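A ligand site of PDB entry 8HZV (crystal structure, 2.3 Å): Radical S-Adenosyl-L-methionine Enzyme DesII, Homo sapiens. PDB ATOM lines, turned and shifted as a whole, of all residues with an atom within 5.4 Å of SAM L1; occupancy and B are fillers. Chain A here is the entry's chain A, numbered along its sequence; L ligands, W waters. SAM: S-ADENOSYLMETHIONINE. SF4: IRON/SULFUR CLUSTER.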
ATOM      1  N   CYS A 141     -30.434  -6.079 -30.351  1.00  0.00           N
ATOM      2  CA  CYS A 141     -30.239  -6.969 -29.224  1.00  0.00           C
ATOM      3  C   CYS A 141     -30.663  -6.257 -27.951  1.00  0.00           C
ATOM      4  O   CYS A 141     -30.542  -5.031 -27.843  1.00  0.00           O
ATOM      5  CB  CYS A 141     -28.789  -7.440 -29.090  1.00  0.00           C
ATOM      6  SG  CYS A 141     -28.630  -8.618 -27.755  1.00  0.00           S
ATOM      7  N   PHE A 147     -18.376  -8.132 -22.571  1.00  0.00           N
ATOM      8  CA  PHE A 147     -17.357  -8.683 -23.453  1.00  0.00           C
ATOM      9  C   PHE A 147     -17.702  -8.586 -24.937  1.00  0.00           C
ATOM     10  O   PHE A 147     -16.863  -8.937 -25.778  1.00  0.00           O
ATOM     11  CB  PHE A 147     -17.091 -10.153 -23.102  1.00  0.00           C
ATOM     12  CG  PHE A 147     -18.334 -10.975 -22.956  1.00  0.00           C
ATOM     13  CD1 PHE A 147     -18.971 -11.507 -24.073  1.00  0.00           C
ATOM     14  CD2 PHE A 147     -18.879 -11.210 -21.708  1.00  0.00           C
ATOM     15  CE1 PHE A 147     -20.122 -12.255 -23.935  1.00  0.00           C
ATOM     16  CE2 PHE A 147     -20.030 -11.958 -21.570  1.00  0.00           C
ATOM     17  CZ  PHE A 147     -20.657 -12.476 -22.684  1.00  0.00           C
ATOM     18  N   CYS A 148     -18.905  -8.133 -25.283  1.00  0.00           N
ATOM     19  CA  CYS A 148     -19.296  -7.995 -26.677  1.00  0.00           C
ATOM     20  C   CYS A 148     -18.876  -6.629 -27.216  1.00  0.00           C
ATOM     21  O   CYS A 148     -18.904  -5.618 -26.510  1.00  0.00           O
ATOM     22  CB  CYS A 148     -20.807  -8.174 -26.830  1.00  0.00           C
ATOM     23  SG  CYS A 148     -21.368  -7.983 -28.530  1.00  0.00           S
ATOM     24  N   SER A 186     -25.861 -16.842 -36.762  1.00  0.00           N
ATOM     25  CA  SER A 186     -25.369 -16.280 -35.515  1.00  0.00           C
ATOM     26  C   SER A 186     -25.580 -14.779 -35.569  1.00  0.00           C
ATOM     27  O   SER A 186     -26.642 -14.311 -35.981  1.00  0.00           O
ATOM     28  CB  SER A 186     -23.901 -16.623 -35.278  1.00  0.00           C
ATOM     29  OG  SER A 186     -23.500 -16.272 -33.973  1.00  0.00           O
ATOM     30  N   GLY A 187     -24.579 -14.007 -35.191  1.00  0.00           N
ATOM     31  CA  GLY A 187     -24.720 -12.591 -35.370  1.00  0.00           C
ATOM     32  C   GLY A 187     -23.521 -11.837 -34.857  1.00  0.00           C
ATOM     33  O   GLY A 187     -22.617 -12.388 -34.210  1.00  0.00           O
ATOM     34  N   GLY A 188     -23.507 -10.561 -35.220  1.00  0.00           N
ATOM     35  CA  GLY A 188     -23.047  -9.564 -34.310  1.00  0.00           C
ATOM     36  C   GLY A 188     -24.132  -9.441 -33.268  1.00  0.00           C
ATOM     37  O   GLY A 188     -23.875  -9.636 -32.070  1.00  0.00           O
ATOM     38  N   LEU A 189     -25.358  -9.195 -33.711  1.00  0.00           N
ATOM     39  CA  LEU A 189     -26.490  -8.958 -32.813  1.00  0.00           C
ATOM     40  C   LEU A 189     -27.268 -10.263 -32.585  1.00  0.00           C
ATOM     41  O   LEU A 189     -26.758 -11.355 -32.824  1.00  0.00           O
ATOM     42  CB  LEU A 189     -27.364  -7.837 -33.381  1.00  0.00           C
ATOM     43  CG  LEU A 189     -26.686  -6.464 -33.475  1.00  0.00           C
ATOM     44  CD1 LEU A 189     -27.684  -5.349 -33.710  1.00  0.00           C
ATOM     45  CD2 LEU A 189     -25.851  -6.188 -32.229  1.00  0.00           C
ATOM     46  N   GLU A 190     -28.512 -10.158 -32.118  1.00  0.00           N
ATOM     47  CA  GLU A 190     -29.285 -11.319 -31.695  1.00  0.00           C
ATOM     48  C   GLU A 190     -30.207 -11.759 -32.814  1.00  0.00           C
ATOM     49  O   GLU A 190     -31.104 -10.995 -33.194  1.00  0.00           O
ATOM     50  CB  GLU A 190     -30.077 -10.997 -30.438  1.00  0.00           C
ATOM     51  CG  GLU A 190     -31.214 -11.958 -30.129  1.00  0.00           C
ATOM     52  CD  GLU A 190     -30.727 -13.381 -29.910  1.00  0.00           C
ATOM     53  OE1 GLU A 190     -29.713 -13.554 -29.201  1.00  0.00           O
ATOM     54  OE2 GLU A 190     -31.352 -14.315 -30.443  1.00  0.00           O
ATOM     55  N   PRO A 191     -30.044 -12.976 -33.349  1.00  0.00           N
ATOM     56  CA  PRO A 191     -30.816 -13.353 -34.548  1.00  0.00           C
ATOM     57  C   PRO A 191     -32.307 -13.505 -34.314  1.00  0.00           C
ATOM     58  O   PRO A 191     -33.090 -13.314 -35.245  1.00  0.00           O
ATOM     59  CB  PRO A 191     -30.167 -14.679 -34.986  1.00  0.00           C
ATOM     60  CG  PRO A 191     -29.492 -15.189 -33.776  1.00  0.00           C
ATOM     61  CD  PRO A 191     -29.043 -13.993 -32.989  1.00  0.00           C
ATOM     62  N   TYR A 214     -27.243 -19.616 -33.064  1.00  0.00           N
ATOM     63  CA  TYR A 214     -26.581 -19.205 -31.825  1.00  0.00           C
ATOM     64  C   TYR A 214     -27.297 -17.972 -31.289  1.00  0.00           C
ATOM     65  O   TYR A 214     -27.336 -16.938 -31.959  1.00  0.00           O
ATOM     66  CB  TYR A 214     -25.096 -18.933 -32.082  1.00  0.00           C
ATOM     67  CG  TYR A 214     -24.342 -20.117 -32.640  1.00  0.00           C
ATOM     68  CD1 TYR A 214     -24.351 -20.388 -34.007  1.00  0.00           C
ATOM     69  CD2 TYR A 214     -23.636 -20.977 -31.812  1.00  0.00           C
ATOM     70  CE1 TYR A 214     -23.666 -21.471 -34.529  1.00  0.00           C
ATOM     71  CE2 TYR A 214     -22.947 -22.066 -32.322  1.00  0.00           C
ATOM     72  CZ  TYR A 214     -22.965 -22.312 -33.675  1.00  0.00           C
ATOM     73  OH  TYR A 214     -22.292 -23.399 -34.179  1.00  0.00           O
ATOM     74  N   THR A 215     -27.866 -18.089 -30.093  1.00  0.00           N
ATOM     75  CA  THR A 215     -28.759 -17.047 -29.585  1.00  0.00           C
ATOM     76  C   THR A 215     -28.614 -16.938 -28.083  1.00  0.00           C
ATOM     77  O   THR A 215     -28.080 -17.830 -27.412  1.00  0.00           O
ATOM     78  CB  THR A 215     -30.220 -17.358 -29.942  1.00  0.00           C
ATOM     79  OG1 THR A 215     -31.088 -16.444 -29.259  1.00  0.00           O
ATOM     80  CG2 THR A 215     -30.576 -18.778 -29.521  1.00  0.00           C
ATOM     81  N   ASN A 216     -29.087 -15.804 -27.535  1.00  0.00           N
ATOM     82  CA  ASN A 216     -29.212 -15.672 -26.095  1.00  0.00           C
ATOM     83  C   ASN A 216     -30.528 -16.224 -25.559  1.00  0.00           C
ATOM     84  O   ASN A 216     -30.688 -16.338 -24.345  1.00  0.00           O
ATOM     85  CB  ASN A 216     -29.032 -14.193 -25.654  1.00  0.00           C
ATOM     86  CG  ASN A 216     -30.116 -13.256 -26.180  1.00  0.00           C
ATOM     87  OD1 ASN A 216     -31.277 -13.631 -26.342  1.00  0.00           O
ATOM     88  ND2 ASN A 216     -29.725 -12.011 -26.443  1.00  0.00           N
ATOM     89  N   ARG A 238     -27.983 -23.307 -30.017  1.00  0.00           N
ATOM     90  CA  ARG A 238     -26.991 -23.158 -28.957  1.00  0.00           C
ATOM     91  C   ARG A 238     -27.258 -21.848 -28.228  1.00  0.00           C
ATOM     92  O   ARG A 238     -27.078 -20.760 -28.792  1.00  0.00           O
ATOM     93  CB  ARG A 238     -25.568 -23.197 -29.511  1.00  0.00           C
ATOM     94  CG  ARG A 238     -24.509 -23.274 -28.415  1.00  0.00           C
ATOM     95  CD  ARG A 238     -23.106 -23.210 -28.970  1.00  0.00           C
ATOM     96  NE  ARG A 238     -22.590 -21.834 -28.983  1.00  0.00           N
ATOM     97  CZ  ARG A 238     -21.353 -21.513 -29.354  1.00  0.00           C
ATOM     98  NH1 ARG A 238     -20.507 -22.453 -29.752  1.00  0.00           N
ATOM     99  NH2 ARG A 238     -20.973 -20.244 -29.327  1.00  0.00           N
ATOM    100  N   SER A 240     -26.259 -19.086 -25.654  1.00  0.00           N
ATOM    101  CA  SER A 240     -25.162 -18.504 -24.884  1.00  0.00           C
ATOM    102  C   SER A 240     -25.639 -18.251 -23.453  1.00  0.00           C
ATOM    103  O   SER A 240     -26.590 -17.493 -23.246  1.00  0.00           O
ATOM    104  CB  SER A 240     -24.683 -17.212 -25.530  1.00  0.00           C
ATOM    105  OG  SER A 240     -24.351 -17.414 -26.886  1.00  0.00           O
ATOM    106  N   TYR A 242     -25.001 -16.822 -19.834  1.00  0.00           N
ATOM    107  CA  TYR A 242     -24.194 -15.757 -19.246  1.00  0.00           C
ATOM    108  C   TYR A 242     -24.268 -15.726 -17.723  1.00  0.00           C
ATOM    109  O   TYR A 242     -23.755 -14.781 -17.112  1.00  0.00           O
ATOM    110  CB  TYR A 242     -24.624 -14.410 -19.824  1.00  0.00           C
ATOM    111  CG  TYR A 242     -24.470 -14.333 -21.336  1.00  0.00           C
ATOM    112  CD1 TYR A 242     -23.315 -14.796 -21.951  1.00  0.00           C
ATOM    113  CD2 TYR A 242     -25.472 -13.807 -22.127  1.00  0.00           C
ATOM    114  CE1 TYR A 242     -23.161 -14.741 -23.320  1.00  0.00           C
ATOM    115  CE2 TYR A 242     -25.333 -13.738 -23.509  1.00  0.00           C
ATOM    116  CZ  TYR A 242     -24.168 -14.198 -24.101  1.00  0.00           C
ATOM    117  OH  TYR A 242     -24.017 -14.135 -25.465  1.00  0.00           O
ATOM    118  N   ALA A 285     -23.353 -22.567 -24.874  1.00  0.00           N
ATOM    119  CA  ALA A 285     -22.014 -22.016 -24.739  1.00  0.00           C
ATOM    120  C   ALA A 285     -21.927 -21.313 -23.403  1.00  0.00           C
ATOM    121  O   ALA A 285     -22.764 -20.452 -23.093  1.00  0.00           O
ATOM    122  CB  ALA A 285     -21.697 -21.045 -25.875  1.00  0.00           C
ATOM    123  N   ILE A 287     -19.248 -19.291 -21.284  1.00  0.00           N
ATOM    124  CA  ILE A 287     -17.987 -18.619 -21.030  1.00  0.00           C
ATOM    125  C   ILE A 287     -17.734 -18.602 -19.530  1.00  0.00           C
ATOM    126  O   ILE A 287     -18.568 -18.131 -18.748  1.00  0.00           O
ATOM    127  CB  ILE A 287     -17.993 -17.201 -21.612  1.00  0.00           C
ATOM    128  CG1 ILE A 287     -18.173 -17.229 -23.130  1.00  0.00           C
ATOM    129  CG2 ILE A 287     -16.716 -16.460 -21.217  1.00  0.00           C
ATOM    130  CD1 ILE A 287     -18.469 -15.858 -23.729  1.00  0.00           C
ATOM    131  N   GLU A 322     -13.992 -19.388 -23.308  1.00  0.00           N
ATOM    132  CA  GLU A 322     -13.232 -18.300 -22.703  1.00  0.00           C
ATOM    133  C   GLU A 322     -13.427 -17.041 -23.529  1.00  0.00           C
ATOM    134  O   GLU A 322     -13.701 -17.117 -24.727  1.00  0.00           O
ATOM    135  CB  GLU A 322     -11.738 -18.649 -22.630  1.00  0.00           C
ATOM    136  CG  GLU A 322     -11.078 -18.398 -21.303  1.00  0.00           C
ATOM    137  CD  GLU A 322      -9.685 -18.990 -21.249  1.00  0.00           C
ATOM    138  OE1 GLU A 322      -8.763 -18.261 -20.843  1.00  0.00           O
ATOM    139  OE2 GLU A 322      -9.522 -20.167 -21.620  1.00  0.00           O
ATOM    140  N   ASP A 323     -13.278 -15.881 -22.887  1.00  0.00           N
ATOM    141  CA  ASP A 323     -13.254 -14.627 -23.627  1.00  0.00           C
ATOM    142  C   ASP A 323     -12.056 -14.626 -24.563  1.00  0.00           C
ATOM    143  O   ASP A 323     -10.911 -14.494 -24.114  1.00  0.00           O
ATOM    144  CB  ASP A 323     -13.196 -13.430 -22.666  1.00  0.00           C
ATOM    145  CG  ASP A 323     -13.341 -12.081 -23.384  1.00  0.00           C
ATOM    146  OD1 ASP A 323     -13.162 -12.015 -24.610  1.00  0.00           O
ATOM    147  OD2 ASP A 323     -13.634 -11.084 -22.695  1.00  0.00           O
ATOM    148  N   TYR A 324     -12.298 -14.787 -25.867  1.00  0.00           N
ATOM    149  CA  TYR A 324     -11.200 -14.861 -26.816  1.00  0.00           C
ATOM    150  C   TYR A 324     -10.594 -13.500 -27.145  1.00  0.00           C
ATOM    151  O   TYR A 324      -9.596 -13.450 -27.870  1.00  0.00           O
ATOM    152  CB  TYR A 324     -11.655 -15.545 -28.123  1.00  0.00           C
ATOM    153  CG  TYR A 324     -12.980 -15.088 -28.680  1.00  0.00           C
ATOM    154  CD1 TYR A 324     -13.202 -13.760 -29.030  1.00  0.00           C
ATOM    155  CD2 TYR A 324     -14.018 -15.987 -28.880  1.00  0.00           C
ATOM    156  CE1 TYR A 324     -14.416 -13.338 -29.539  1.00  0.00           C
ATOM    157  CE2 TYR A 324     -15.241 -15.579 -29.394  1.00  0.00           C
ATOM    158  CZ  TYR A 324     -15.430 -14.252 -29.721  1.00  0.00           C
ATOM    159  OH  TYR A 324     -16.641 -13.838 -30.236  1.00  0.00           O
ATOM    160  N   SER A 325     -11.173 -12.415 -26.622  1.00  0.00           N
ATOM    161  CA  SER A 325     -10.595 -11.097 -26.873  1.00  0.00           C
ATOM    162  C   SER A 325      -9.328 -10.872 -26.046  1.00  0.00           C
ATOM    163  O   SER A 325      -8.413 -10.186 -26.498  1.00  0.00           O
ATOM    164  CB  SER A 325     -11.627 -10.009 -26.554  1.00  0.00           C
ATOM    165  OG  SER A 325     -11.805  -9.870 -25.159  1.00  0.00           O
ATOM    166  N   ARG A 327      -9.248  -9.147 -23.294  1.00  0.00           N
ATOM    167  CA  ARG A 327      -9.395  -7.953 -22.477  1.00  0.00           C
ATOM    168  C   ARG A 327      -9.675  -8.347 -21.018  1.00  0.00           C
ATOM    169  O   ARG A 327     -10.249  -9.410 -20.746  1.00  0.00           O
ATOM    170  CB  ARG A 327     -10.505  -7.052 -23.020  1.00  0.00           C
ATOM    171  CG  ARG A 327     -10.184  -6.480 -24.408  1.00  0.00           C
ATOM    172  CD  ARG A 327     -11.354  -5.686 -24.991  1.00  0.00           C
ATOM    173  NE  ARG A 327     -12.602  -6.440 -24.924  1.00  0.00           N
ATOM    174  CZ  ARG A 327     -13.232  -6.956 -25.980  1.00  0.00           C
ATOM    175  NH1 ARG A 327     -12.742  -6.804 -27.201  1.00  0.00           N
ATOM    176  NH2 ARG A 327     -14.364  -7.627 -25.795  1.00  0.00           N
ATOM    177  N   GLU A 408     -16.137 -10.629 -35.562  1.00  0.00           N
ATOM    178  CA  GLU A 408     -16.502  -9.552 -34.637  1.00  0.00           C
ATOM    179  C   GLU A 408     -16.453  -8.173 -35.285  1.00  0.00           C
ATOM    180  O   GLU A 408     -16.464  -7.162 -34.569  1.00  0.00           O
ATOM    181  CB  GLU A 408     -15.585  -9.571 -33.415  1.00  0.00           C
ATOM    182  CG  GLU A 408     -15.600 -10.892 -32.637  1.00  0.00           C
ATOM    183  CD  GLU A 408     -17.005 -11.387 -32.362  1.00  0.00           C
ATOM    184  OE1 GLU A 408     -17.360 -12.477 -32.854  1.00  0.00           O
ATOM    185  OE2 GLU A 408     -17.753 -10.677 -31.648  1.00  0.00           O
ATOM    186  N   PHE A 411     -20.804  -5.581 -36.899  1.00  0.00           N
ATOM    187  CA  PHE A 411     -21.664  -4.882 -35.963  1.00  0.00           C
ATOM    188  C   PHE A 411     -21.974  -3.500 -36.504  1.00  0.00           C
ATOM    189  O   PHE A 411     -21.075  -2.803 -36.987  1.00  0.00           O
ATOM    190  CB  PHE A 411     -21.009  -4.751 -34.578  1.00  0.00           C
ATOM    191  CG  PHE A 411     -20.847  -6.064 -33.848  1.00  0.00           C
ATOM    192  CD1 PHE A 411     -19.822  -6.935 -34.170  1.00  0.00           C
ATOM    193  CD2 PHE A 411     -21.702  -6.404 -32.824  1.00  0.00           C
ATOM    194  CE1 PHE A 411     -19.662  -8.126 -33.488  1.00  0.00           C
ATOM    195  CE2 PHE A 411     -21.550  -7.592 -32.130  1.00  0.00           C
ATOM    196  CZ  PHE A 411     -20.529  -8.457 -32.465  1.00  0.00           C
HETATM  197  N   SAM L   1     -26.890 -12.386 -29.421  1.00  0.00           N
HETATM  198  CA  SAM L   1     -26.599 -13.759 -29.792  1.00  0.00           C
HETATM  199  C   SAM L   1     -25.901 -14.505 -28.641  1.00  0.00           C
HETATM  200  O   SAM L   1     -25.916 -15.737 -28.565  1.00  0.00           O
HETATM  201  OXT SAM L   1     -25.311 -13.914 -27.741  1.00  0.00           O
HETATM  202  CB  SAM L   1     -25.736 -13.774 -31.056  1.00  0.00           C
HETATM  203  CG  SAM L   1     -24.443 -14.533 -30.856  1.00  0.00           C
HETATM  204  SD  SAM L   1     -22.912 -13.714 -31.364  1.00  0.00           S
HETATM  205  CE  SAM L   1     -22.438 -12.577 -30.038  1.00  0.00           C
HETATM  206  C5' SAM L   1     -21.763 -15.135 -31.365  1.00  0.00           C
HETATM  207  C4' SAM L   1     -21.197 -15.773 -30.085  1.00  0.00           C
HETATM  208  O4' SAM L   1     -20.007 -15.136 -29.689  1.00  0.00           O
HETATM  209  C3' SAM L   1     -22.100 -15.838 -28.854  1.00  0.00           C
HETATM  210  O3' SAM L   1     -22.241 -17.173 -28.466  1.00  0.00           O
HETATM  211  C2' SAM L   1     -21.355 -15.059 -27.784  1.00  0.00           C
HETATM  212  O2' SAM L   1     -21.513 -15.662 -26.515  1.00  0.00           O
HETATM  213  C1' SAM L   1     -19.924 -15.141 -28.278  1.00  0.00           C
HETATM  214  N9  SAM L   1     -19.046 -14.035 -27.886  1.00  0.00           N
HETATM  215  C8  SAM L   1     -19.235 -12.701 -28.121  1.00  0.00           C
HETATM  216  N7  SAM L   1     -18.163 -12.034 -27.619  1.00  0.00           N
HETATM  217  C5  SAM L   1     -17.295 -12.930 -27.090  1.00  0.00           C
HETATM  218  C6  SAM L   1     -16.067 -12.788 -26.459  1.00  0.00           C
HETATM  219  N6  SAM L   1     -15.528 -11.589 -26.295  1.00  0.00           N
HETATM  220  N1  SAM L   1     -15.398 -13.910 -26.017  1.00  0.00           N
HETATM  221  C2  SAM L   1     -15.955 -15.159 -26.192  1.00  0.00           C
HETATM  222  N3  SAM L   1     -17.187 -15.293 -26.818  1.00  0.00           N
HETATM  223  C4  SAM L   1     -17.841 -14.187 -27.264  1.00  0.00           C
HETATM  224 FE1  SF4 L   2     -24.512 -10.334 -25.583  1.00  0.00          FE
HETATM  225 FE2  SF4 L   2     -23.537  -9.272 -27.833  1.00  0.00          FE
HETATM  226 FE3  SF4 L   2     -26.145  -9.096 -27.317  1.00  0.00          FE
HETATM  227 FE4  SF4 L   2     -25.039 -11.513 -27.988  1.00  0.00          FE
HETATM  228  S1  SF4 L   2     -25.179  -9.647 -29.330  1.00  0.00           S
HETATM  229  S2  SF4 L   2     -26.505 -11.089 -26.257  1.00  0.00           S
HETATM  230  S3  SF4 L   2     -23.047 -11.345 -27.006  1.00  0.00           S
HETATM  231  S4  SF4 L   2     -24.545  -8.109 -26.136  1.00  0.00           S
HETATM  232  O   HOH W   1     -20.869 -17.781 -25.109  1.00  0.00           O
HETATM  233  O   HOH W   2     -18.020  -9.437 -29.238  1.00  0.00           O
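The side-chain hydroxyl of Tyr 242 sits at hydrogen-bond distance from an oxygen (O2') of SAM L1 (3.1 Å).
The side-chain hydroxyl (OG) of Ser 240 lies within hydrogen-bond range of an oxygen (O3') of SAM L1.
The side-chain carboxylate (OD1) of Asp 323 lies within hydrogen-bond range of a nitrogen (N6) of SAM L1 (2.9 Å).
The backbone NH (N) of Thr 215 sits close to an oxygen (O) of SAM L1 (3.4 Å).
N6 of SAM L1 is in hydrogen-bond range of O of Phe 147, 3.0 Å away.
A nitrogen (N) of SAM L1 sits close to the side-chain carboxylate (OE1) of Glu 190, at 3.1 Å.
The backbone NH of Tyr 324 is in hydrogen-bond range of a nitrogen (N1) of SAM L1, at 3.2 Å.
An oxygen (O) of SAM L1 lies within hydrogen-bond range of the backbone NH of Asn 216 (3.3 Å).
O3' of SAM L1 sits at hydrogen-bond distance from NH2 of Arg 238 (3.4 Å).
The side-chain hydroxyl (OH) of Tyr 242 lies close to a sulfur (S3) of SF4 L2, 3.3 Å away.
S2 of SF4 L2 lies close to ND2 of Asn 216, at 3.4 Å.
FE2 of SF4 L2 is bound by SG of Cys 148 (2.6 Å).
SG of Cys 141 is bound to FE3 of SF4 L2.
FE4 of SF4 L2 is bound by OXT of SAM L1 (2.4 Å).
The backbone carbonyl oxygen of Thr 215 is in hydrogen-bond range of the backbone NH of Ser 240 (2.8 Å).
OG of Ser 325 is in hydrogen-bond range of OD1 of Asp 323.
The side-chain hydroxyl (OG1) of Thr 215 is in hydrogen-bond range of the side-chain carboxylate (OE2) of Glu 190 (2.5 Å).
The backbone NH (N) of Thr 215 lies within hydrogen-bond range of the backbone carbonyl oxygen (O) of Arg 238 (3.1 Å).
O of Phe 147 sits at hydrogen-bond distance from NH2 of Arg 327, 2.8 Å away.
The side-chain carboxylate of Glu 190 is in hydrogen-bond range of the backbone NH of Asn 216 (2.9 Å).
The side-chain hydroxyl (OH) of Tyr 324 lies within hydrogen-bond range of the side-chain carboxylate (OE1) of Glu 408, at 3.0 Å.
The side-chain sulfur (SG) of Cys 141 lies close to the side-chain amide nitrogen (ND2) of Asn 216 (3.8 Å).
SD of SAM L1 sits close to OG of Ser 186, at 3.7 Å.
SD of SAM L1 lies close to O of Gly 187 (3.2 Å).
Merely in contact with SAM L1: Gly 188 (3.9 Å), Leu 189 (3.2 Å), Pro 191 (3.8 Å), Tyr 214 (3.7 Å), Ile 287 (3.4 Å) and Glu 322 (3.3 Å).
Hydrophobic or aromatic side chains within 4 Å of SAM L1: Phe 147, Pro 191, Tyr 242, Ile 287 and Tyr 324.
17 residues have an atom within 4 Å of SAM L1: Phe 147, Ser 186, Gly 187, Gly 188, Leu 189, Glu 190, Pro 191, Tyr 214, Thr 215, Asn 216, Arg 238, Ser 240, Tyr 242, Ile 287, Glu 322, Asp 323 and Tyr 324.
Along chain A the residues within 4 Å of SAM L1 span positions 147 to 324.
Water W2 bridges OE2 of Glu 408 (2.7 Å) and N7 of SAM L1 (3.1 Å).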
